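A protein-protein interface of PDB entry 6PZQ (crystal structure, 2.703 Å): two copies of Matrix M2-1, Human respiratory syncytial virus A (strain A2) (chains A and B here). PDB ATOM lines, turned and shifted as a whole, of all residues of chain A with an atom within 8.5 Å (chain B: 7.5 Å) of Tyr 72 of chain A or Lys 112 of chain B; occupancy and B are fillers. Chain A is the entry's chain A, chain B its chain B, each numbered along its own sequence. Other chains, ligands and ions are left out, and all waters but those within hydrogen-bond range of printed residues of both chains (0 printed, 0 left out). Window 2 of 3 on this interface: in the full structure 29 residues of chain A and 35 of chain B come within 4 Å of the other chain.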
ATOM      1  N   LYS A  48      27.238  -2.394  13.485  1.00  0.00           N
ATOM      2  CA  LYS A  48      27.038  -2.351  14.932  1.00  0.00           C
ATOM      3  C   LYS A  48      26.764  -3.752  15.492  1.00  0.00           C
ATOM      4  O   LYS A  48      27.331  -4.142  16.511  1.00  0.00           O
ATOM      5  CB  LYS A  48      25.913  -1.367  15.227  1.00  0.00           C
ATOM      6  CG  LYS A  48      25.815  -0.866  16.682  1.00  0.00           C
ATOM      7  CD  LYS A  48      25.527   0.672  16.783  1.00  0.00           C
ATOM      8  CE  LYS A  48      24.048   1.006  17.132  1.00  0.00           C
ATOM      9  NZ  LYS A  48      23.822   2.452  17.580  1.00  0.00           N
ATOM     10  N   THR A  69      27.512  11.383  28.745  1.00  0.00           N
ATOM     11  CA  THR A  69      26.679  12.431  28.154  1.00  0.00           C
ATOM     12  C   THR A  69      27.540  13.663  27.809  1.00  0.00           C
ATOM     13  O   THR A  69      27.418  14.243  26.713  1.00  0.00           O
ATOM     14  CB  THR A  69      25.499  12.825  29.110  1.00  0.00           C
ATOM     15  OG1 THR A  69      24.871  14.030  28.649  1.00  0.00           O
ATOM     16  CG2 THR A  69      25.983  13.043  30.545  1.00  0.00           C
ATOM     17  N   GLU A  70      28.412  14.032  28.762  1.00  0.00           N
ATOM     18  CA  GLU A  70      29.385  15.115  28.568  1.00  0.00           C
ATOM     19  C   GLU A  70      30.516  14.707  27.620  1.00  0.00           C
ATOM     20  O   GLU A  70      31.085  15.560  26.931  1.00  0.00           O
ATOM     21  CB  GLU A  70      29.954  15.552  29.926  1.00  0.00           C
ATOM     22  CG  GLU A  70      30.543  14.404  30.812  1.00  0.00           C
ATOM     23  CD  GLU A  70      29.496  13.623  31.647  1.00  0.00           C
ATOM     24  OE1 GLU A  70      28.437  14.182  32.034  1.00  0.00           O
ATOM     25  OE2 GLU A  70      29.742  12.426  31.916  1.00  0.00           O
ATOM     26  N   GLU A  71      30.823  13.406  27.554  1.00  0.00           N
ATOM     27  CA  GLU A  71      31.835  12.862  26.653  1.00  0.00           C
ATOM     28  C   GLU A  71      31.337  12.752  25.206  1.00  0.00           C
ATOM     29  O   GLU A  71      32.134  12.884  24.263  1.00  0.00           O
ATOM     30  CB  GLU A  71      32.290  11.485  27.176  1.00  0.00           C
ATOM     31  CG  GLU A  71      33.071  11.484  28.522  1.00  0.00           C
ATOM     32  CD  GLU A  71      33.444  10.063  29.042  1.00  0.00           C
ATOM     33  OE1 GLU A  71      32.944   9.048  28.476  1.00  0.00           O
ATOM     34  OE2 GLU A  71      34.242   9.962  30.011  1.00  0.00           O
ATOM     35  N   TYR A  72      30.032  12.520  25.011  1.00  0.00           N
ATOM     36  CA  TYR A  72      29.444  12.517  23.664  1.00  0.00           C
ATOM     37  C   TYR A  72      29.378  13.918  23.062  1.00  0.00           C
ATOM     38  O   TYR A  72      29.511  14.074  21.847  1.00  0.00           O
ATOM     39  CB  TYR A  72      28.042  11.915  23.701  1.00  0.00           C
ATOM     40  CG  TYR A  72      27.900  10.631  22.943  1.00  0.00           C
ATOM     41  CD1 TYR A  72      28.384   9.427  23.485  1.00  0.00           C
ATOM     42  CD2 TYR A  72      27.273  10.604  21.692  1.00  0.00           C
ATOM     43  CE1 TYR A  72      28.258   8.229  22.792  1.00  0.00           C
ATOM     44  CE2 TYR A  72      27.141   9.412  20.978  1.00  0.00           C
ATOM     45  CZ  TYR A  72      27.634   8.226  21.529  1.00  0.00           C
ATOM     46  OH  TYR A  72      27.497   7.046  20.803  1.00  0.00           O
ATOM     47  N   ALA A  73      29.106  14.941  23.874  1.00  0.00           N
ATOM     48  CA  ALA A  73      29.312  16.299  23.396  1.00  0.00           C
ATOM     49  C   ALA A  73      30.609  16.342  22.610  1.00  0.00           C
ATOM     50  O   ALA A  73      30.631  16.688  21.419  1.00  0.00           O
ATOM     51  CB  ALA A  73      29.361  17.284  24.578  1.00  0.00           C
ATOM     52  N   LEU A  74      31.677  15.901  23.294  1.00  0.00           N
ATOM     53  CA  LEU A  74      33.054  15.980  22.805  1.00  0.00           C
ATOM     54  C   LEU A  74      33.252  15.179  21.537  1.00  0.00           C
ATOM     55  O   LEU A  74      33.764  15.694  20.532  1.00  0.00           O
ATOM     56  CB  LEU A  74      34.026  15.431  23.865  1.00  0.00           C
ATOM     57  CG  LEU A  74      34.691  16.284  24.944  1.00  0.00           C
ATOM     58  CD1 LEU A  74      34.873  17.704  24.434  1.00  0.00           C
ATOM     59  CD2 LEU A  74      33.899  16.228  26.206  1.00  0.00           C
ATOM     60  N   GLY A  75      32.908  13.892  21.597  1.00  0.00           N
ATOM     61  CA  GLY A  75      33.285  12.954  20.572  1.00  0.00           C
ATOM     62  C   GLY A  75      34.522  12.197  20.981  1.00  0.00           C
ATOM     63  O   GLY A  75      35.116  12.448  22.015  1.00  0.00           O
ATOM     64  N   VAL A  76      34.950  11.258  20.146  1.00  0.00           N
ATOM     65  CA  VAL A  76      36.141  10.502  20.526  1.00  0.00           C
ATOM     66  C   VAL A  76      37.390  11.347  20.290  1.00  0.00           C
ATOM     67  O   VAL A  76      38.306  11.329  21.110  1.00  0.00           O
ATOM     68  CB  VAL A  76      36.207   9.129  19.804  1.00  0.00           C
ATOM     69  CG1 VAL A  76      37.537   8.523  19.934  1.00  0.00           C
ATOM     70  CG2 VAL A  76      35.251   8.127  20.431  1.00  0.00           C
ATOM     71  N   GLY A  78      37.547  14.615  20.428  1.00  0.00           N
ATOM     72  CA  GLY A  78      37.568  15.618  21.469  1.00  0.00           C
ATOM     73  C   GLY A  78      37.996  15.066  22.812  1.00  0.00           C
ATOM     74  O   GLY A  78      38.724  15.730  23.547  1.00  0.00           O
ATOM     75  N   VAL A  79      37.553  13.855  23.167  1.00  0.00           N
ATOM     76  CA  VAL A  79      38.051  13.265  24.414  1.00  0.00           C
ATOM     77  C   VAL A  79      39.491  12.789  24.300  1.00  0.00           C
ATOM     78  O   VAL A  79      40.147  12.570  25.317  1.00  0.00           O
ATOM     79  CB  VAL A  79      37.245  12.058  24.951  1.00  0.00           C
ATOM     80  CG1 VAL A  79      35.771  12.388  25.086  1.00  0.00           C
ATOM     81  CG2 VAL A  79      37.464  10.862  24.107  1.00  0.00           C
ATOM     82  N   LYS A 101      38.519   2.463  19.897  1.00  0.00           N
ATOM     83  CA  LYS A 101      37.403   2.962  19.098  1.00  0.00           C
ATOM     84  C   LYS A 101      37.867   3.769  17.900  1.00  0.00           C
ATOM     85  O   LYS A 101      37.267   3.687  16.831  1.00  0.00           O
ATOM     86  CB  LYS A 101      36.465   3.814  19.945  1.00  0.00           C
ATOM     87  CG  LYS A 101      35.280   3.042  20.524  1.00  0.00           C
ATOM     88  CD  LYS A 101      34.266   3.995  21.123  1.00  0.00           C
ATOM     89  CE  LYS A 101      34.177   3.910  22.638  1.00  0.00           C
ATOM     90  NZ  LYS A 101      34.160   5.293  23.226  1.00  0.00           N
ATOM     91  N   ASN B 107      18.090   2.846  17.688  1.00  0.00           N
ATOM     92  CA  ASN B 107      19.543   2.881  17.772  1.00  0.00           C
ATOM     93  C   ASN B 107      19.925   3.928  18.818  1.00  0.00           C
ATOM     94  O   ASN B 107      19.560   5.105  18.705  1.00  0.00           O
ATOM     95  CB  ASN B 107      20.184   3.095  16.374  1.00  0.00           C
ATOM     96  CG  ASN B 107      20.558   4.543  16.065  1.00  0.00           C
ATOM     97  OD1 ASN B 107      21.733   4.907  16.130  1.00  0.00           O
ATOM     98  ND2 ASN B 107      19.576   5.352  15.667  1.00  0.00           N
ATOM     99  N   SER B 108      20.635   3.466  19.856  1.00  0.00           N
ATOM    100  CA  SER B 108      21.011   4.310  20.984  1.00  0.00           C
ATOM    101  C   SER B 108      21.670   5.606  20.545  1.00  0.00           C
ATOM    102  O   SER B 108      21.526   6.626  21.223  1.00  0.00           O
ATOM    103  CB  SER B 108      21.934   3.529  21.914  1.00  0.00           C
ATOM    104  OG  SER B 108      22.436   2.399  21.228  1.00  0.00           O
ATOM    105  N   ASP B 109      22.359   5.617  19.406  1.00  0.00           N
ATOM    106  CA  ASP B 109      23.103   6.826  19.045  1.00  0.00           C
ATOM    107  C   ASP B 109      22.184   8.022  18.813  1.00  0.00           C
ATOM    108  O   ASP B 109      22.513   9.141  19.223  1.00  0.00           O
ATOM    109  CB  ASP B 109      23.986   6.570  17.827  1.00  0.00           C
ATOM    110  CG  ASP B 109      25.326   5.970  18.208  1.00  0.00           C
ATOM    111  OD1 ASP B 109      26.114   6.695  18.864  1.00  0.00           O
ATOM    112  OD2 ASP B 109      25.576   4.781  17.882  1.00  0.00           O
ATOM    113  N   ASP B 110      21.019   7.820  18.180  1.00  0.00           N
ATOM    114  CA  ASP B 110      20.163   8.974  17.902  1.00  0.00           C
ATOM    115  C   ASP B 110      19.317   9.380  19.104  1.00  0.00           C
ATOM    116  O   ASP B 110      18.666  10.429  19.049  1.00  0.00           O
ATOM    117  CB  ASP B 110      19.252   8.726  16.681  1.00  0.00           C
ATOM    118  CG  ASP B 110      19.031  10.022  15.816  1.00  0.00           C
ATOM    119  OD1 ASP B 110      18.987  11.163  16.362  1.00  0.00           O
ATOM    120  OD2 ASP B 110      18.916   9.899  14.572  1.00  0.00           O
ATOM    121  N   ILE B 111      19.331   8.598  20.187  1.00  0.00           N
ATOM    122  CA  ILE B 111      18.851   9.088  21.478  1.00  0.00           C
ATOM    123  C   ILE B 111      19.882  10.005  22.114  1.00  0.00           C
ATOM    124  O   ILE B 111      19.581  11.137  22.513  1.00  0.00           O
ATOM    125  CB  ILE B 111      18.534   7.914  22.418  1.00  0.00           C
ATOM    126  CG1 ILE B 111      17.299   7.160  21.955  1.00  0.00           C
ATOM    127  CG2 ILE B 111      18.328   8.413  23.815  1.00  0.00           C
ATOM    128  CD1 ILE B 111      17.639   6.153  20.861  1.00  0.00           C
ATOM    129  N   LYS B 112      21.114   9.508  22.239  1.00  0.00           N
ATOM    130  CA  LYS B 112      22.217  10.332  22.717  1.00  0.00           C
ATOM    131  C   LYS B 112      22.293  11.645  21.960  1.00  0.00           C
ATOM    132  O   LYS B 112      22.528  12.703  22.552  1.00  0.00           O
ATOM    133  CB  LYS B 112      23.528   9.579  22.571  1.00  0.00           C
ATOM    134  CG  LYS B 112      23.459   8.125  22.955  1.00  0.00           C
ATOM    135  CD  LYS B 112      24.637   7.704  23.749  1.00  0.00           C
ATOM    136  CE  LYS B 112      24.786   6.231  23.748  1.00  0.00           C
ATOM    137  NZ  LYS B 112      25.219   5.703  22.434  1.00  0.00           N
ATOM    138  N   LYS B 113      22.098  11.602  20.649  1.00  0.00           N
ATOM    139  CA  LYS B 113      21.970  12.849  19.918  1.00  0.00           C
ATOM    140  C   LYS B 113      20.942  13.769  20.569  1.00  0.00           C
ATOM    141  O   LYS B 113      21.243  14.916  20.906  1.00  0.00           O
ATOM    142  CB  LYS B 113      21.587  12.589  18.461  1.00  0.00           C
ATOM    143  CG  LYS B 113      21.257  13.889  17.716  1.00  0.00           C
ATOM    144  CD  LYS B 113      22.420  14.887  17.850  1.00  0.00           C
ATOM    145  CE  LYS B 113      22.030  16.317  17.564  1.00  0.00           C
ATOM    146  NZ  LYS B 113      22.709  17.271  18.534  1.00  0.00           N
ATOM    147  N   LEU B 114      19.713  13.277  20.753  1.00  0.00           N
ATOM    148  CA  LEU B 114      18.623  14.131  21.237  1.00  0.00           C
ATOM    149  C   LEU B 114      18.860  14.582  22.670  1.00  0.00           C
ATOM    150  O   LEU B 114      18.532  15.715  23.033  1.00  0.00           O
ATOM    151  CB  LEU B 114      17.288  13.387  21.161  1.00  0.00           C
ATOM    152  CG  LEU B 114      16.697  12.890  19.834  1.00  0.00           C
ATOM    153  CD1 LEU B 114      15.605  11.917  20.146  1.00  0.00           C
ATOM    154  CD2 LEU B 114      16.146  14.003  18.978  1.00  0.00           C
ATOM    155  N   ARG B 115      19.452  13.715  23.474  1.00  0.00           N
ATOM    156  CA  ARG B 115      19.679  13.988  24.903  1.00  0.00           C
ATOM    157  C   ARG B 115      20.692  15.103  25.028  1.00  0.00           C
ATOM    158  O   ARG B 115      20.646  15.812  25.998  1.00  0.00           O
ATOM    159  CB  ARG B 115      20.196  12.750  25.622  1.00  0.00           C
ATOM    160  CG  ARG B 115      20.808  13.040  26.980  1.00  0.00           C
ATOM    161  CD  ARG B 115      21.512  11.840  27.554  1.00  0.00           C
ATOM    162  NE  ARG B 115      22.631  11.497  26.717  1.00  0.00           N
ATOM    163  CZ  ARG B 115      23.479  10.538  26.974  1.00  0.00           C
ATOM    164  NH1 ARG B 115      23.354   9.829  28.068  1.00  0.00           N
ATOM    165  NH2 ARG B 115      24.458  10.314  26.136  1.00  0.00           N
ATOM    166  N   ASP B 116      21.563  15.248  24.040  1.00  0.00           N
ATOM    167  CA  ASP B 116      22.627  16.265  24.033  1.00  0.00           C
ATOM    168  C   ASP B 116      22.138  17.615  23.532  1.00  0.00           C
ATOM    169  O   ASP B 116      22.907  18.551  23.609  1.00  0.00           O
ATOM    170  CB  ASP B 116      23.805  15.756  23.232  1.00  0.00           C
ATOM    171  CG  ASP B 116      25.027  15.781  24.098  1.00  0.00           C
ATOM    172  OD1 ASP B 116      25.242  16.814  24.722  1.00  0.00           O
ATOM    173  OD2 ASP B 116      25.662  14.734  24.219  1.00  0.00           O
ATOM    174  N   ASN B 117      20.890  17.727  23.096  1.00  0.00           N
ATOM    175  CA  ASN B 117      20.285  18.993  22.642  1.00  0.00           C
ATOM    176  C   ASN B 117      19.497  19.690  23.728  1.00  0.00           C
ATOM    177  O   ASN B 117      18.883  20.678  23.400  1.00  0.00           O
ATOM    178  CB  ASN B 117      19.286  18.740  21.526  1.00  0.00           C
ATOM    179  CG  ASN B 117      20.009  18.287  20.294  1.00  0.00           C
ATOM    180  OD1 ASN B 117      21.223  18.365  20.272  1.00  0.00           O
ATOM    181  ND2 ASN B 117      19.287  17.840  19.286  1.00  0.00           N
ATOM    182  N   TYR B 128      15.667   9.759  28.691  1.00  0.00           N
ATOM    183  CA  TYR B 128      16.566   9.382  27.610  1.00  0.00           C
ATOM    184  C   TYR B 128      17.611   8.341  28.007  1.00  0.00           C
ATOM    185  O   TYR B 128      18.098   7.631  27.131  1.00  0.00           O
ATOM    186  CB  TYR B 128      17.210  10.649  27.075  1.00  0.00           C
ATOM    187  CG  TYR B 128      16.304  11.289  26.084  1.00  0.00           C
ATOM    188  CD1 TYR B 128      14.999  11.591  26.413  1.00  0.00           C
ATOM    189  CD2 TYR B 128      16.712  11.515  24.810  1.00  0.00           C
ATOM    190  CE1 TYR B 128      14.135  12.139  25.501  1.00  0.00           C
ATOM    191  CE2 TYR B 128      15.862  12.066  23.885  1.00  0.00           C
ATOM    192  CZ  TYR B 128      14.577  12.383  24.227  1.00  0.00           C
ATOM    193  OH  TYR B 128      13.746  12.942  23.266  1.00  0.00           O
ATOM    194  N   ASN B 129      17.939   8.181  29.288  1.00  0.00           N
ATOM    195  CA  ASN B 129      18.946   7.197  29.672  1.00  0.00           C
ATOM    196  C   ASN B 129      18.377   5.840  30.073  1.00  0.00           C
ATOM    197  O   ASN B 129      19.085   4.826  29.964  1.00  0.00           O
ATOM    198  CB  ASN B 129      19.793   7.732  30.840  1.00  0.00           C
ATOM    199  CG  ASN B 129      20.772   8.835  30.421  1.00  0.00           C
ATOM    200  OD1 ASN B 129      21.680   8.631  29.605  1.00  0.00           O
ATOM    201  ND2 ASN B 129      20.597  10.004  30.999  1.00  0.00           N
ATOM    202  N   VAL B 131      15.931   4.431  28.452  1.00  0.00           N
ATOM    203  CA  VAL B 131      15.791   3.819  27.122  1.00  0.00           C
ATOM    204  C   VAL B 131      17.126   3.301  26.622  1.00  0.00           C
ATOM    205  O   VAL B 131      17.233   2.150  26.187  1.00  0.00           O
ATOM    206  CB  VAL B 131      15.186   4.808  26.109  1.00  0.00           C
ATOM    207  CG1 VAL B 131      13.698   5.004  26.351  1.00  0.00           C
ATOM    208  CG2 VAL B 131      15.898   6.126  26.192  1.00  0.00           C
ATOM    209  N   ILE B 132      18.166   4.131  26.690  1.00  0.00           N
ATOM    210  CA  ILE B 132      19.486   3.683  26.256  1.00  0.00           C
ATOM    211  C   ILE B 132      19.953   2.462  27.062  1.00  0.00           C
ATOM    212  O   ILE B 132      20.499   1.505  26.492  1.00  0.00           O
ATOM    213  CB  ILE B 132      20.496   4.843  26.304  1.00  0.00           C
ATOM    214  CG1 ILE B 132      19.973   6.033  25.504  1.00  0.00           C
ATOM    215  CG2 ILE B 132      21.729   4.458  25.608  1.00  0.00           C
ATOM    216  CD1 ILE B 132      20.768   7.240  25.706  1.00  0.00           C
ATOM    217  N   GLU B 136      20.365  -1.104  25.257  1.00  0.00           N
ATOM    218  CA  GLU B 136      21.676  -1.731  25.452  1.00  0.00           C
ATOM    219  C   GLU B 136      21.590  -3.047  26.217  1.00  0.00           C
ATOM    220  O   GLU B 136      22.234  -4.028  25.846  1.00  0.00           O
ATOM    221  CB  GLU B 136      22.606  -0.770  26.174  1.00  0.00           C
ATOM    222  CG  GLU B 136      23.160   0.256  25.270  1.00  0.00           C
ATOM    223  CD  GLU B 136      23.863  -0.395  24.111  1.00  0.00           C
ATOM    224  OE1 GLU B 136      24.500  -1.452  24.344  1.00  0.00           O
ATOM    225  OE2 GLU B 136      23.738   0.112  22.973  1.00  0.00           O
ATOM    226  N   ARG B 139      20.277  -5.490  23.739  1.00  0.00           N
ATOM    227  CA  ARG B 139      21.207  -5.933  22.697  1.00  0.00           C
ATOM    228  C   ARG B 139      22.089  -7.078  23.178  1.00  0.00           C
ATOM    229  O   ARG B 139      22.338  -8.037  22.439  1.00  0.00           O
ATOM    230  CB  ARG B 139      22.096  -4.785  22.212  1.00  0.00           C
ATOM    231  CG  ARG B 139      23.260  -5.314  21.314  1.00  0.00           C
ATOM    232  CD  ARG B 139      24.061  -4.252  20.524  1.00  0.00           C
ATOM    233  NE  ARG B 139      23.239  -3.185  19.929  1.00  0.00           N
ATOM    234  CZ  ARG B 139      23.333  -1.880  20.224  1.00  0.00           C
ATOM    235  NH1 ARG B 139      24.230  -1.452  21.106  1.00  0.00           N
ATOM    236  NH2 ARG B 139      22.537  -0.986  19.628  1.00  0.00           N
ATOM    237  N   ILE B 171      12.075  10.481  16.642  1.00  0.00           N
ATOM    238  CA  ILE B 171      13.255  10.244  15.810  1.00  0.00           C
ATOM    239  C   ILE B 171      12.908  10.219  14.328  1.00  0.00           C
ATOM    240  O   ILE B 171      13.665  10.713  13.483  1.00  0.00           O
ATOM    241  CB  ILE B 171      13.942   8.935  16.213  1.00  0.00           C
ATOM    242  CG1 ILE B 171      14.704   9.132  17.524  1.00  0.00           C
ATOM    243  CG2 ILE B 171      14.866   8.490  15.081  1.00  0.00           C
ATOM    244  CD1 ILE B 171      15.368   7.841  18.031  1.00  0.00           C
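The backbone carbonyl oxygen (O) of Thr 69 of chain A lies close to the side-chain carboxylate (OD2) of Asp 116 of chain B.
The side-chain amino group of Lys 112 of chain B is in hydrogen-bond range of the side-chain hydroxyl of Tyr 72 of chain A (3.1 Å).
OH of Tyr 72 of chain A is in hydrogen-bond range of OD1 of Asp 109 of chain B, at 2.4 Å.
OD2 of Asp 116 of chain B is in hydrogen-bond range of N of Ala 73 of chain A (3.5 Å).
NZ of Lys 48 of chain A lies within salt-bridge range of OD2 of Asp 109 of chain B, at 2.9 Å.
The side-chain amide oxygen (OD1) of Asn 107 of chain B lies close to the backbone NH (N) of Asp 109 of chain B, 3.4 Å away.
NH1 of Arg 115 of chain B sits at hydrogen-bond distance from OD1 of Asn 129 of chain B (2.6 Å).
The side-chain hydroxyl (OG) of Ser 108 of chain B sits at hydrogen-bond distance from the side-chain carboxylate (OE2) of Glu 136 of chain B (3.2 Å).
OE2 of Glu 136 of chain B lies within salt-bridge range of NH1 of Arg 139 of chain B (2.5 Å).
The side-chain carboxylate of Asp 109 of chain B is in salt-bridge range of the side-chain amino group of Lys 112 of chain B, at 3.8 Å.
Lys 48 of chain A touches Asn 107 of chain B.
Lys 48 of chain A touches Ser 108 of chain B (NZ to OG, 3.9 Å).
Lys 48 of chain A touches Arg 139 of chain B.
Thr 69 of chain A touches Arg 115 of chain B.
Asp 116 of chain B touches Tyr 72 of chain A (OD2 to CB, 3.7 Å).
Of the printed residues of chain B, Ala 73 of chain A touches Asp 116.
Of the printed residues of chain A, Asn 107 of chain B touches Lys 48 (3.5 Å).
Of the printed residues of chain A, Ser 108 of chain B touches Lys 48 (3.9 Å).
Printed residues of chain A within 4 Å of Asp 109 of chain B: Lys 48 and Tyr 72.
Lys 112 of chain B touches just one residue of chain A: Tyr 72 (3.1 Å).
Of the printed residues of chain A, Arg 115 of chain B touches Thr 69.
Asn 117 of chain B touches none of the printed residues of chain A.
Asn 129 of chain B touches none of the printed residues of chain A.
The nearest residue of chain A that does not touch Lys 112 of chain B is Lys 48 of chain A (6.0 Å).
Of the 18 printed residues of chain B, 7 touch a printed residue of chain A.
Printed residues of chain B that touch a printed residue of chain A: Asn 107, Ser 108, Asp 109, Lys 112, Arg 115, Asp 116 and Arg 139.
Of the 12 printed residues of chain A, 4 touch a printed residue of chain B.
Printed residues of chain A that touch a printed residue of chain B: Lys 48, Thr 69, Tyr 72 and Ala 73.
Hydrophobic or aromatic side chains of chain A that line the printed part of chain B: Tyr 72.
Among the printed residues, Asp or Glu carboxylates within 4 Å of a Lys or Arg side-chain nitrogen of the other chain: Lys 48 of chain A with Asp 109 of chain B.
No position is printed for both chains.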
